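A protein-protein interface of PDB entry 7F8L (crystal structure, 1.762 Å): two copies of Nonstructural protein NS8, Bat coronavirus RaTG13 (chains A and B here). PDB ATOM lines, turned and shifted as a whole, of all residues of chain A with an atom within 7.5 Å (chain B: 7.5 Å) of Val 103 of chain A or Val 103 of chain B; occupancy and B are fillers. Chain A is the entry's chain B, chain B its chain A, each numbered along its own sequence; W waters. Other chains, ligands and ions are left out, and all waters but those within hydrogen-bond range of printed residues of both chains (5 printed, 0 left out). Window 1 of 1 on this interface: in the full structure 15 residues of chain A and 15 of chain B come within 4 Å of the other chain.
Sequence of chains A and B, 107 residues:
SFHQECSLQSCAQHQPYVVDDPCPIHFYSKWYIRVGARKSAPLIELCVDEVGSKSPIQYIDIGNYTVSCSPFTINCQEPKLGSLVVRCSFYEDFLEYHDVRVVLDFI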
ATOM      1  N   CYS A   6     -27.427 -33.255   8.559  1.00  0.00           N
ATOM      2  CA  CYS A   6     -27.210 -32.087   7.710  1.00  0.00           C
ATOM      3  C   CYS A   6     -26.833 -30.901   8.582  1.00  0.00           C
ATOM      4  O   CYS A   6     -27.507 -30.646   9.586  1.00  0.00           O
ATOM      5  CB  CYS A   6     -28.483 -31.745   6.932  1.00  0.00           C
ATOM      6  SG  CYS A   6     -28.145 -30.809   5.463  1.00  0.00           S
ATOM      7  N   SER A   7     -25.763 -30.192   8.218  1.00  0.00           N
ATOM      8  CA  SER A   7     -25.365 -28.970   8.916  1.00  0.00           C
ATOM      9  C   SER A   7     -25.385 -27.809   7.932  1.00  0.00           C
ATOM     10  O   SER A   7     -24.677 -27.834   6.918  1.00  0.00           O
ATOM     11  CB  SER A   7     -23.979 -29.113   9.554  1.00  0.00           C
ATOM     12  OG  SER A   7     -23.493 -27.856  10.025  1.00  0.00           O
ATOM     13  N   LEU A   8     -26.182 -26.790   8.233  1.00  0.00           N
ATOM     14  CA  LEU A   8     -26.291 -25.617   7.382  1.00  0.00           C
ATOM     15  C   LEU A   8     -25.498 -24.482   8.023  1.00  0.00           C
ATOM     16  O   LEU A   8     -25.736 -24.127   9.181  1.00  0.00           O
ATOM     17  CB  LEU A   8     -27.752 -25.222   7.185  1.00  0.00           C
ATOM     18  CG  LEU A   8     -28.028 -23.994   6.320  1.00  0.00           C
ATOM     19  CD1 LEU A   8     -27.512 -24.203   4.902  1.00  0.00           C
ATOM     20  CD2 LEU A   8     -29.514 -23.692   6.306  1.00  0.00           C
ATOM     21  N   GLN A   9     -24.553 -23.924   7.272  1.00  0.00           N
ATOM     22  CA  GLN A   9     -23.670 -22.888   7.779  1.00  0.00           C
ATOM     23  C   GLN A   9     -23.649 -21.723   6.804  1.00  0.00           C
ATOM     24  O   GLN A   9     -23.916 -21.889   5.615  1.00  0.00           O
ATOM     25  CB  GLN A   9     -22.269 -23.436   8.010  1.00  0.00           C
ATOM     26  CG  GLN A   9     -22.261 -24.589   9.001  1.00  0.00           C
ATOM     27  CD  GLN A   9     -20.877 -25.069   9.357  1.00  0.00           C
ATOM     28  OE1 GLN A   9     -19.920 -24.303   9.339  1.00  0.00           O
ATOM     29  NE2 GLN A   9     -20.766 -26.343   9.711  1.00  0.00           N
ATOM     30  N   SER A  10     -23.362 -20.534   7.323  1.00  0.00           N
ATOM     31  CA  SER A  10     -23.384 -19.316   6.522  1.00  0.00           C
ATOM     32  C   SER A  10     -21.993 -18.700   6.453  1.00  0.00           C
ATOM     33  O   SER A  10     -21.314 -18.576   7.474  1.00  0.00           O
ATOM     34  CB  SER A  10     -24.365 -18.302   7.109  1.00  0.00           C
ATOM     35  OG  SER A  10     -25.651 -18.880   7.248  1.00  0.00           O
ATOM     36  N   CYS A  11     -21.582 -18.294   5.255  1.00  0.00           N
ATOM     37  CA  CYS A  11     -20.321 -17.576   5.109  1.00  0.00           C
ATOM     38  C   CYS A  11     -20.384 -16.688   3.875  1.00  0.00           C
ATOM     39  O   CYS A  11     -21.243 -16.863   3.008  1.00  0.00           O
ATOM     40  CB  CYS A  11     -19.129 -18.542   5.009  1.00  0.00           C
ATOM     41  SG  CYS A  11     -19.318 -19.910   3.805  1.00  0.00           S
ATOM     42  N   TYR A  17     -13.255 -19.144   5.497  1.00  0.00           N
ATOM     43  CA  TYR A  17     -14.273 -19.528   6.465  1.00  0.00           C
ATOM     44  C   TYR A  17     -13.773 -20.728   7.249  1.00  0.00           C
ATOM     45  O   TYR A  17     -13.495 -21.781   6.666  1.00  0.00           O
ATOM     46  CB  TYR A  17     -15.605 -19.865   5.785  1.00  0.00           C
ATOM     47  CG  TYR A  17     -16.667 -20.348   6.741  1.00  0.00           C
ATOM     48  CD1 TYR A  17     -17.160 -19.509   7.743  1.00  0.00           C
ATOM     49  CD2 TYR A  17     -17.168 -21.649   6.663  1.00  0.00           C
ATOM     50  CE1 TYR A  17     -18.128 -19.947   8.629  1.00  0.00           C
ATOM     51  CE2 TYR A  17     -18.153 -22.099   7.548  1.00  0.00           C
ATOM     52  CZ  TYR A  17     -18.631 -21.238   8.521  1.00  0.00           C
ATOM     53  OH  TYR A  17     -19.589 -21.671   9.410  1.00  0.00           O
ATOM     54  N   ALA A  37     -21.880 -36.259  -4.675  1.00  0.00           N
ATOM     55  CA  ALA A  37     -22.928 -36.407  -3.653  1.00  0.00           C
ATOM     56  C   ALA A  37     -23.693 -37.720  -3.810  1.00  0.00           C
ATOM     57  O   ALA A  37     -24.871 -37.813  -3.444  1.00  0.00           O
ATOM     58  CB  ALA A  37     -23.901 -35.217  -3.648  1.00  0.00           C
ATOM     59  N   GLU A  78     -19.439 -23.816  -2.538  1.00  0.00           N
ATOM     60  CA  GLU A  78     -19.786 -25.237  -2.561  1.00  0.00           C
ATOM     61  C   GLU A  78     -18.787 -25.995  -3.425  1.00  0.00           C
ATOM     62  O   GLU A  78     -18.386 -25.507  -4.484  1.00  0.00           O
ATOM     63  CB  GLU A  78     -21.193 -25.466  -3.096  1.00  0.00           C
ATOM     64  CG  GLU A  78     -22.301 -25.020  -2.153  1.00  0.00           C
ATOM     65  CD  GLU A  78     -22.480 -25.864  -0.867  1.00  0.00           C
ATOM     66  OE1 GLU A  78     -21.741 -26.827  -0.604  1.00  0.00           O
ATOM     67  OE2 GLU A  78     -23.398 -25.539  -0.112  1.00  0.00           O
ATOM     68  N   PRO A  79     -18.347 -27.167  -2.984  1.00  0.00           N
ATOM     69  CA  PRO A  79     -17.377 -27.925  -3.780  1.00  0.00           C
ATOM     70  C   PRO A  79     -18.024 -28.476  -5.042  1.00  0.00           C
ATOM     71  O   PRO A  79     -19.196 -28.866  -5.054  1.00  0.00           O
ATOM     72  CB  PRO A  79     -16.932 -29.052  -2.835  1.00  0.00           C
ATOM     73  CG  PRO A  79     -17.817 -28.941  -1.594  1.00  0.00           C
ATOM     74  CD  PRO A  79     -18.914 -27.969  -1.890  1.00  0.00           C
ATOM     75  N   SER A  83     -19.943 -33.526  -2.396  1.00  0.00           N
ATOM     76  CA  SER A  83     -20.443 -32.875  -1.197  1.00  0.00           C
ATOM     77  C   SER A  83     -19.384 -32.906  -0.095  1.00  0.00           C
ATOM     78  O   SER A  83     -18.485 -33.744  -0.088  1.00  0.00           O
ATOM     79  CB  SER A  83     -21.720 -33.568  -0.728  1.00  0.00           C
ATOM     80  OG  SER A  83     -21.495 -34.963  -0.631  1.00  0.00           O
ATOM     81  N   LEU A  84     -19.513 -31.988   0.854  1.00  0.00           N
ATOM     82  CA  LEU A  84     -18.616 -31.930   2.002  1.00  0.00           C
ATOM     83  C   LEU A  84     -19.257 -32.704   3.147  1.00  0.00           C
ATOM     84  O   LEU A  84     -20.385 -32.396   3.561  1.00  0.00           O
ATOM     85  CB  LEU A  84     -18.359 -30.486   2.416  1.00  0.00           C
ATOM     86  CG  LEU A  84     -17.430 -30.324   3.623  1.00  0.00           C
ATOM     87  CD1 LEU A  84     -16.061 -30.888   3.299  1.00  0.00           C
ATOM     88  CD2 LEU A  84     -17.353 -28.849   4.057  1.00  0.00           C
ATOM     89  N   VAL A 100     -22.140 -36.305   8.758  1.00  0.00           N
ATOM     90  CA  VAL A 100     -22.924 -35.082   8.649  1.00  0.00           C
ATOM     91  C   VAL A 100     -22.487 -34.366   7.377  1.00  0.00           C
ATOM     92  O   VAL A 100     -21.291 -34.126   7.177  1.00  0.00           O
ATOM     93  CB  VAL A 100     -22.746 -34.167   9.876  1.00  0.00           C
ATOM     94  CG1 VAL A 100     -23.650 -32.928   9.764  1.00  0.00           C
ATOM     95  CG2 VAL A 100     -23.044 -34.939  11.160  1.00  0.00           C
ATOM     96  N   ARG A 101     -23.441 -34.046   6.518  1.00  0.00           N
ATOM     97  CA  ARG A 101     -23.132 -33.259   5.332  1.00  0.00           C
ATOM     98  C   ARG A 101     -23.189 -31.782   5.684  1.00  0.00           C
ATOM     99  O   ARG A 101     -24.092 -31.339   6.398  1.00  0.00           O
ATOM    100  CB  ARG A 101     -24.105 -33.571   4.200  1.00  0.00           C
ATOM    101  CG  ARG A 101     -23.843 -32.711   2.962  1.00  0.00           C
ATOM    102  CD  ARG A 101     -24.492 -33.315   1.773  1.00  0.00           C
ATOM    103  NE  ARG A 101     -24.469 -32.401   0.643  1.00  0.00           N
ATOM    104  CZ  ARG A 101     -25.109 -32.638  -0.494  1.00  0.00           C
ATOM    105  NH1 ARG A 101     -25.793 -33.763  -0.633  1.00  0.00           N
ATOM    106  NH2 ARG A 101     -25.046 -31.760  -1.493  1.00  0.00           N
ATOM    107  N   VAL A 102     -22.216 -31.016   5.196  1.00  0.00           N
ATOM    108  CA  VAL A 102     -22.148 -29.585   5.473  1.00  0.00           C
ATOM    109  C   VAL A 102     -22.516 -28.838   4.206  1.00  0.00           C
ATOM    110  O   VAL A 102     -21.940 -29.094   3.144  1.00  0.00           O
ATOM    111  CB  VAL A 102     -20.754 -29.167   5.973  1.00  0.00           C
ATOM    112  CG1 VAL A 102     -20.660 -27.632   6.074  1.00  0.00           C
ATOM    113  CG2 VAL A 102     -20.461 -29.817   7.327  1.00  0.00           C
ATOM    114  N   VAL A 103     -23.483 -27.932   4.311  1.00  0.00           N
ATOM    115  CA  VAL A 103     -23.922 -27.138   3.173  1.00  0.00           C
ATOM    116  C   VAL A 103     -23.932 -25.672   3.592  1.00  0.00           C
ATOM    117  O   VAL A 103     -24.040 -25.355   4.781  1.00  0.00           O
ATOM    118  CB  VAL A 103     -25.301 -27.630   2.666  1.00  0.00           C
ATOM    119  CG1 VAL A 103     -26.358 -27.349   3.659  1.00  0.00           C
ATOM    120  CG2 VAL A 103     -25.653 -27.033   1.345  1.00  0.00           C
ATOM    121  N   LEU A 104     -23.769 -24.774   2.613  1.00  0.00           N
ATOM    122  CA  LEU A 104     -23.502 -23.367   2.881  1.00  0.00           C
ATOM    123  C   LEU A 104     -24.604 -22.493   2.317  1.00  0.00           C
ATOM    124  O   LEU A 104     -24.952 -22.618   1.139  1.00  0.00           O
ATOM    125  CB  LEU A 104     -22.157 -22.929   2.270  1.00  0.00           C
ATOM    126  CG  LEU A 104     -20.929 -23.744   2.705  1.00  0.00           C
ATOM    127  CD1 LEU A 104     -19.722 -23.293   1.899  1.00  0.00           C
ATOM    128  CD2 LEU A 104     -20.667 -23.599   4.193  1.00  0.00           C
ATOM    129  N   ASP A 105     -25.128 -21.596   3.154  1.00  0.00           N
ATOM    130  CA  ASP A 105     -25.855 -20.421   2.696  1.00  0.00           C
ATOM    131  C   ASP A 105     -24.880 -19.249   2.600  1.00  0.00           C
ATOM    132  O   ASP A 105     -23.985 -19.103   3.436  1.00  0.00           O
ATOM    133  CB  ASP A 105     -27.003 -20.078   3.656  1.00  0.00           C
ATOM    134  CG  ASP A 105     -28.250 -20.917   3.408  1.00  0.00           C
ATOM    135  OD1 ASP A 105     -28.294 -21.663   2.399  1.00  0.00           O
ATOM    136  OD2 ASP A 105     -29.202 -20.823   4.221  1.00  0.00           O
ATOM    137  N   PHE A 106     -25.047 -18.405   1.586  1.00  0.00           N
ATOM    138  CA  PHE A 106     -24.070 -17.352   1.318  1.00  0.00           C
ATOM    139  C   PHE A 106     -24.594 -15.993   1.762  1.00  0.00           C
ATOM    140  O   PHE A 106     -25.711 -15.603   1.405  1.00  0.00           O
ATOM    141  CB  PHE A 106     -23.703 -17.344  -0.158  1.00  0.00           C
ATOM    142  CG  PHE A 106     -23.102 -18.633  -0.610  1.00  0.00           C
ATOM    143  CD1 PHE A 106     -21.884 -19.051  -0.095  1.00  0.00           C
ATOM    144  CD2 PHE A 106     -23.759 -19.441  -1.528  1.00  0.00           C
ATOM    145  CE1 PHE A 106     -21.312 -20.253  -0.499  1.00  0.00           C
ATOM    146  CE2 PHE A 106     -23.202 -20.651  -1.935  1.00  0.00           C
ATOM    147  CZ  PHE A 106     -21.977 -21.063  -1.418  1.00  0.00           C
ATOM    148  N   GLU B   5     -31.435 -24.755   9.975  1.00  0.00           N
ATOM    149  CA  GLU B   5     -32.032 -26.079   9.853  1.00  0.00           C
ATOM    150  C   GLU B   5     -31.951 -26.615   8.424  1.00  0.00           C
ATOM    151  O   GLU B   5     -32.206 -25.900   7.436  1.00  0.00           O
ATOM    152  CB  GLU B   5     -33.483 -26.116  10.336  1.00  0.00           C
ATOM    153  CG  GLU B   5     -33.893 -27.532  10.723  1.00  0.00           C
ATOM    154  CD  GLU B   5     -35.278 -27.626  11.329  1.00  0.00           C
ATOM    155  OE1 GLU B   5     -35.721 -26.651  11.975  1.00  0.00           O
ATOM    156  OE2 GLU B   5     -35.920 -28.688  11.160  1.00  0.00           O
ATOM    157  N   CYS B   6     -31.639 -27.908   8.348  1.00  0.00           N
ATOM    158  CA  CYS B   6     -31.182 -28.614   7.162  1.00  0.00           C
ATOM    159  C   CYS B   6     -31.878 -29.962   7.107  1.00  0.00           C
ATOM    160  O   CYS B   6     -31.956 -30.641   8.130  1.00  0.00           O
ATOM    161  CB  CYS B   6     -29.676 -28.852   7.254  1.00  0.00           C
ATOM    162  SG  CYS B   6     -28.874 -28.920   5.711  1.00  0.00           S
ATOM    163  N   SER B   7     -32.363 -30.366   5.930  1.00  0.00           N
ATOM    164  CA  SER B   7     -32.945 -31.695   5.755  1.00  0.00           C
ATOM    165  C   SER B   7     -32.233 -32.425   4.627  1.00  0.00           C
ATOM    166  O   SER B   7     -32.355 -32.032   3.466  1.00  0.00           O
ATOM    167  CB  SER B   7     -34.440 -31.626   5.442  1.00  0.00           C
ATOM    168  OG  SER B   7     -34.941 -32.938   5.206  1.00  0.00           O
ATOM    169  N   LEU B   8     -31.549 -33.520   4.960  1.00  0.00           N
ATOM    170  CA  LEU B   8     -30.850 -34.331   3.966  1.00  0.00           C
ATOM    171  C   LEU B   8     -31.703 -35.533   3.571  1.00  0.00           C
ATOM    172  O   LEU B   8     -32.123 -36.313   4.433  1.00  0.00           O
ATOM    173  CB  LEU B   8     -29.503 -34.805   4.522  1.00  0.00           C
ATOM    174  CG  LEU B   8     -28.691 -35.729   3.619  1.00  0.00           C
ATOM    175  CD1 LEU B   8     -28.340 -35.006   2.310  1.00  0.00           C
ATOM    176  CD2 LEU B   8     -27.437 -36.229   4.346  1.00  0.00           C
ATOM    177  N   GLN B   9     -31.933 -35.699   2.274  1.00  0.00           N
ATOM    178  CA  GLN B   9     -32.793 -36.758   1.754  1.00  0.00           C
ATOM    179  C   GLN B   9     -32.090 -37.464   0.604  1.00  0.00           C
ATOM    180  O   GLN B   9     -31.272 -36.862  -0.089  1.00  0.00           O
ATOM    181  CB  GLN B   9     -34.128 -36.189   1.272  1.00  0.00           C
ATOM    182  CG  GLN B   9     -34.810 -35.343   2.352  1.00  0.00           C
ATOM    183  CD  GLN B   9     -36.221 -34.873   2.011  1.00  0.00           C
ATOM    184  OE1 GLN B   9     -36.905 -35.425   1.138  1.00  0.00           O
ATOM    185  NE2 GLN B   9     -36.666 -33.847   2.726  1.00  0.00           N
ATOM    186  N   SER B  10     -32.406 -38.746   0.404  1.00  0.00           N
ATOM    187  CA  SER B  10     -31.812 -39.523  -0.677  1.00  0.00           C
ATOM    188  C   SER B  10     -32.866 -39.858  -1.722  1.00  0.00           C
ATOM    189  O   SER B  10     -34.006 -40.189  -1.384  1.00  0.00           O
ATOM    190  CB  SER B  10     -31.189 -40.831  -0.171  1.00  0.00           C
ATOM    191  OG  SER B  10     -30.123 -40.586   0.727  1.00  0.00           O
ATOM    192  N   CYS B  11     -32.485 -39.799  -2.989  1.00  0.00           N
ATOM    193  CA  CYS B  11     -33.426 -40.156  -4.041  1.00  0.00           C
ATOM    194  C   CYS B  11     -32.665 -40.655  -5.252  1.00  0.00           C
ATOM    195  O   CYS B  11     -31.461 -40.410  -5.409  1.00  0.00           O
ATOM    196  CB  CYS B  11     -34.328 -38.983  -4.454  1.00  0.00           C
ATOM    197  SG  CYS B  11     -33.517 -37.403  -4.851  1.00  0.00           S
ATOM    198  N   TYR B  17     -39.272 -37.633  -7.520  1.00  0.00           N
ATOM    199  CA  TYR B  17     -39.059 -37.855  -6.094  1.00  0.00           C
ATOM    200  C   TYR B  17     -40.118 -37.076  -5.330  1.00  0.00           C
ATOM    201  O   TYR B  17     -40.175 -35.851  -5.444  1.00  0.00           O
ATOM    202  CB  TYR B  17     -37.656 -37.413  -5.652  1.00  0.00           C
ATOM    203  CG  TYR B  17     -37.464 -37.514  -4.153  1.00  0.00           C
ATOM    204  CD1 TYR B  17     -37.695 -38.718  -3.490  1.00  0.00           C
ATOM    205  CD2 TYR B  17     -37.073 -36.416  -3.399  1.00  0.00           C
ATOM    206  CE1 TYR B  17     -37.535 -38.820  -2.121  1.00  0.00           C
ATOM    207  CE2 TYR B  17     -36.901 -36.514  -2.018  1.00  0.00           C
ATOM    208  CZ  TYR B  17     -37.131 -37.719  -1.389  1.00  0.00           C
ATOM    209  OH  TYR B  17     -36.976 -37.818  -0.018  1.00  0.00           O
ATOM    210  N   ALA B  37     -28.412 -19.684  -3.549  1.00  0.00           N
ATOM    211  CA  ALA B  37     -28.323 -19.975  -2.119  1.00  0.00           C
ATOM    212  C   ALA B  37     -27.848 -18.754  -1.328  1.00  0.00           C
ATOM    213  O   ALA B  37     -27.228 -18.892  -0.267  1.00  0.00           O
ATOM    214  CB  ALA B  37     -27.418 -21.191  -1.846  1.00  0.00           C
ATOM    215  N   PRO B  79     -29.541 -29.114  -7.345  1.00  0.00           N
ATOM    216  CA  PRO B  79     -30.115 -27.765  -7.486  1.00  0.00           C
ATOM    217  C   PRO B  79     -29.115 -26.817  -8.144  1.00  0.00           C
ATOM    218  O   PRO B  79     -27.949 -26.753  -7.745  1.00  0.00           O
ATOM    219  CB  PRO B  79     -30.413 -27.364  -6.039  1.00  0.00           C
ATOM    220  CG  PRO B  79     -29.377 -28.126  -5.225  1.00  0.00           C
ATOM    221  CD  PRO B  79     -29.063 -29.397  -5.979  1.00  0.00           C
ATOM    222  N   SER B  83     -30.823 -22.885  -3.858  1.00  0.00           N
ATOM    223  CA  SER B  83     -31.169 -23.907  -2.878  1.00  0.00           C
ATOM    224  C   SER B  83     -32.673 -24.144  -2.855  1.00  0.00           C
ATOM    225  O   SER B  83     -33.471 -23.226  -3.072  1.00  0.00           O
ATOM    226  CB  SER B  83     -30.691 -23.506  -1.474  1.00  0.00           C
ATOM    227  OG  SER B  83     -30.992 -22.147  -1.200  1.00  0.00           O
ATOM    228  N   LEU B  84     -33.056 -25.385  -2.577  1.00  0.00           N
ATOM    229  CA  LEU B  84     -34.457 -25.723  -2.327  1.00  0.00           C
ATOM    230  C   LEU B  84     -34.783 -25.466  -0.857  1.00  0.00           C
ATOM    231  O   LEU B  84     -34.106 -25.986   0.033  1.00  0.00           O
ATOM    232  CB  LEU B  84     -34.726 -27.178  -2.703  1.00  0.00           C
ATOM    233  CG  LEU B  84     -36.174 -27.653  -2.582  1.00  0.00           C
ATOM    234  CD1 LEU B  84     -37.060 -26.830  -3.519  1.00  0.00           C
ATOM    235  CD2 LEU B  84     -36.279 -29.155  -2.897  1.00  0.00           C
ATOM    236  N   VAL B 100     -36.452 -24.323   6.123  1.00  0.00           N
ATOM    237  CA  VAL B 100     -35.605 -25.510   6.130  1.00  0.00           C
ATOM    238  C   VAL B 100     -35.083 -25.721   4.716  1.00  0.00           C
ATOM    239  O   VAL B 100     -35.865 -25.766   3.763  1.00  0.00           O
ATOM    240  CB  VAL B 100     -36.378 -26.754   6.610  1.00  0.00           C
ATOM    241  CG1 VAL B 100     -35.449 -27.969   6.700  1.00  0.00           C
ATOM    242  CG2 VAL B 100     -37.074 -26.475   7.931  1.00  0.00           C
ATOM    243  N   ARG B 101     -33.771 -25.853   4.584  1.00  0.00           N
ATOM    244  CA  ARG B 101     -33.181 -26.205   3.304  1.00  0.00           C
ATOM    245  C   ARG B 101     -33.211 -27.716   3.095  1.00  0.00           C
ATOM    246  O   ARG B 101     -32.947 -28.486   4.019  1.00  0.00           O
ATOM    247  CB  ARG B 101     -31.747 -25.693   3.249  1.00  0.00           C
ATOM    248  CG  ARG B 101     -31.076 -25.939   1.932  1.00  0.00           C
ATOM    249  CD  ARG B 101     -29.854 -25.104   1.827  1.00  0.00           C
ATOM    250  NE  ARG B 101     -29.066 -25.492   0.669  1.00  0.00           N
ATOM    251  CZ  ARG B 101     -27.947 -24.886   0.315  1.00  0.00           C
ATOM    252  NH1 ARG B 101     -27.506 -23.857   1.027  1.00  0.00           N
ATOM    253  NH2 ARG B 101     -27.281 -25.306  -0.755  1.00  0.00           N
ATOM    254  N   VAL B 102     -33.554 -28.135   1.876  1.00  0.00           N
ATOM    255  CA  VAL B 102     -33.616 -29.548   1.515  1.00  0.00           C
ATOM    256  C   VAL B 102     -32.430 -29.828   0.613  1.00  0.00           C
ATOM    257  O   VAL B 102     -32.282 -29.206  -0.441  1.00  0.00           O
ATOM    258  CB  VAL B 102     -34.944 -29.918   0.839  1.00  0.00           C
ATOM    259  CG1 VAL B 102     -34.919 -31.350   0.331  1.00  0.00           C
ATOM    260  CG2 VAL B 102     -36.092 -29.741   1.834  1.00  0.00           C
ATOM    261  N   VAL B 103     -31.600 -30.777   1.043  1.00  0.00           N
ATOM    262  CA  VAL B 103     -30.373 -31.203   0.383  1.00  0.00           C
ATOM    263  C   VAL B 103     -30.551 -32.655  -0.051  1.00  0.00           C
ATOM    264  O   VAL B 103     -31.134 -33.456   0.696  1.00  0.00           O
ATOM    265  CB  VAL B 103     -29.192 -31.070   1.372  1.00  0.00           C
ATOM    266  CG1 VAL B 103     -27.906 -31.499   0.749  1.00  0.00           C
ATOM    267  CG2 VAL B 103     -29.098 -29.633   1.891  1.00  0.00           C
ATOM    268  N   LEU B 104     -30.043 -33.000  -1.239  1.00  0.00           N
ATOM    269  CA  LEU B 104     -30.194 -34.342  -1.800  1.00  0.00           C
ATOM    270  C   LEU B 104     -28.860 -35.075  -1.888  1.00  0.00           C
ATOM    271  O   LEU B 104     -27.890 -34.541  -2.442  1.00  0.00           O
ATOM    272  CB  LEU B 104     -30.818 -34.279  -3.195  1.00  0.00           C
ATOM    273  CG  LEU B 104     -32.218 -33.675  -3.302  1.00  0.00           C
ATOM    274  CD1 LEU B 104     -32.713 -33.791  -4.753  1.00  0.00           C
ATOM    275  CD2 LEU B 104     -33.192 -34.305  -2.318  1.00  0.00           C
ATOM    276  N   ASP B 105     -28.821 -36.296  -1.340  1.00  0.00           N
ATOM    277  CA  ASP B 105     -27.836 -37.310  -1.700  1.00  0.00           C
ATOM    278  C   ASP B 105     -28.451 -38.229  -2.748  1.00  0.00           C
ATOM    279  O   ASP B 105     -29.652 -38.513  -2.717  1.00  0.00           O
ATOM    280  CB  ASP B 105     -27.412 -38.152  -0.492  1.00  0.00           C
ATOM    281  CG  ASP B 105     -26.365 -37.473   0.380  1.00  0.00           C
ATOM    282  OD1 ASP B 105     -25.721 -36.488  -0.062  1.00  0.00           O
ATOM    283  OD2 ASP B 105     -26.169 -37.960   1.516  1.00  0.00           O
ATOM    284  N   PHE B 106     -27.637 -38.703  -3.676  1.00  0.00           N
ATOM    285  CA  PHE B 106     -28.133 -39.536  -4.762  1.00  0.00           C
ATOM    286  C   PHE B 106     -27.834 -41.013  -4.506  1.00  0.00           C
ATOM    287  O   PHE B 106     -26.709 -41.385  -4.149  1.00  0.00           O
ATOM    288  CB  PHE B 106     -27.542 -39.063  -6.091  1.00  0.00           C
ATOM    289  CG  PHE B 106     -27.803 -37.605  -6.349  1.00  0.00           C
ATOM    290  CD1 PHE B 106     -29.102 -37.159  -6.510  1.00  0.00           C
ATOM    291  CD2 PHE B 106     -26.770 -36.683  -6.353  1.00  0.00           C
ATOM    292  CE1 PHE B 106     -29.382 -35.812  -6.708  1.00  0.00           C
ATOM    293  CE2 PHE B 106     -27.030 -35.321  -6.543  1.00  0.00           C
ATOM    294  CZ  PHE B 106     -28.347 -34.886  -6.724  1.00  0.00           C
HETATM  295  O   HOH W   1     -26.668 -32.351  -3.780  1.00  0.00           O
HETATM  296  O   HOH W   2     -30.935 -21.724   1.371  1.00  0.00           O
HETATM  297  O   HOH W   3     -23.343 -36.353   0.962  1.00  0.00           O
HETATM  298  O   HOH W   4     -29.774 -28.911  10.405  1.00  0.00           O
HETATM  299  O   HOH W   5     -24.841 -23.936  -1.254  1.00  0.00           O
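NH1 of Arg 101 of chain B is in hydrogen-bond range of O of Leu 104 of chain A (2.8 Å). SG of Cys 6 of chain B is disulfide-bonded to SG of Cys 6 of chain A, at 2.0 Å. NH1 of Arg 101 of chain B lies within salt-bridge range of OD1 of Asp 105 of chain A, 2.7 Å away. N of Phe 106 of chain A sits at hydrogen-bond distance from O of Ala 37 of chain B, at 2.9 Å. The backbone NH (N) of Phe 106 of chain B is in hydrogen-bond range of the backbone carbonyl oxygen (O) of Ala 37 of chain A, at 2.9 Å. NH1 of Arg 101 of chain A sits at hydrogen-bond distance from O of Leu 104 of chain B (2.9 Å). The side-chain carboxylate (OE2) of Glu 78 of chain A is in salt-bridge range of the guanidinium group (NH2) of Arg 101 of chain B, at 3.9 Å. The side-chain carboxylate (OD1) of Asp 105 of chain B is in salt-bridge range of the guanidinium group (NH1) of Arg 101 of chain A (2.8 Å).
O of Arg 101 of chain A sits at hydrogen-bond distance from N of Ser 7 of chain A (2.7 Å). The backbone carbonyl oxygen (O) of Ser 7 of chain A is in hydrogen-bond range of the backbone NH (N) of Val 103 of chain A. O of Val 103 of chain A sits at hydrogen-bond distance from N of Gln 9 of chain A (2.9 Å).
SG of Cys 6 of chain A touches CG2 of Val 103 of chain B (3.9 Å). Glu 5 of chain B touches Leu 8 of chain A (O to CD2, 3.7 Å). CD1 of Leu 8 of chain A touches NH1 of Arg 101 of chain B (3.9 Å). Val 103 of chain B touches Arg 101 of chain A. Val 103 of chain A touches Arg 101 of chain B. CG1 of Val 103 of chain A touches CG2 of Val 103 of chain B, at 3.98 Å.
Printed residues of chain B within 4 Å of Arg 101 of chain A: Val 103 (3.3 Å), Leu 104 (2.9 Å) and Asp 105 (2.8 Å). Printed residues of chain A within 4 Å of Val 103 of chain B: Cys 6 (3.9 Å), Arg 101 (3.3 Å) and Val 103 (3.98 Å). Of the printed residues of chain A, Phe 106 of chain B touches Ala 37 (2.9 Å). The nearest printed residue of chain B that does not touch Val 103 of chain A is Ser 83 of chain B (6.8 Å). The nearest printed residue of chain A that does not touch Val 103 of chain B is Leu 8 of chain A (6.4 Å).
Printed residues of chain A that touch a printed residue of chain B: Cys 6, Leu 8, Ala 37, Glu 78, Arg 101, Val 103, Leu 104, Asp 105 and Phe 106. Hydrophobic or aromatic side chains of chain A within 4 Å of the printed part of chain B: Leu 8, Val 103 and Phe 106. Printed residues of chain B that touch a printed residue of chain A: Glu 5, Cys 6, Ala 37, Arg 101, Val 103, Leu 104, Asp 105 and Phe 106. Hydrophobic or aromatic side chains of chain B that line the printed part of chain A: Val 103 and Phe 106. Among the printed residues, 17 pairs touch across the chains. Among the printed residues, Asp or Glu carboxylates within 4 Å of a Lys or Arg side-chain nitrogen of the other chain: Glu 78 of chain A with Arg 101 of chain B, Arg 101 of chain A with Asp 105 of chain B and Asp 105 of chain A with Arg 101 of chain B.
Leu 8 of chain A touches Arg 101 of chain B, but with the chains exchanged Arg 101 of chain A does not touch Leu 8 of chain B (4.1 Å). Ala 37 of chain A touches Phe 106 of chain B, and with the chains exchanged Phe 106 of chain A touches Ala 37 of chain B.
Water W2 lies within hydrogen-bond range of OG of Ser 83 of chain B (2.6 Å) and OD1 of Asp 105 of chain A (2.8 Å). Water W1 bridges O of Leu 104 of chain B and NH2 of Arg 101 of chain A. Water W4 bridges N of Cys 6 of chain B and O of Cys 6 of chain A.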
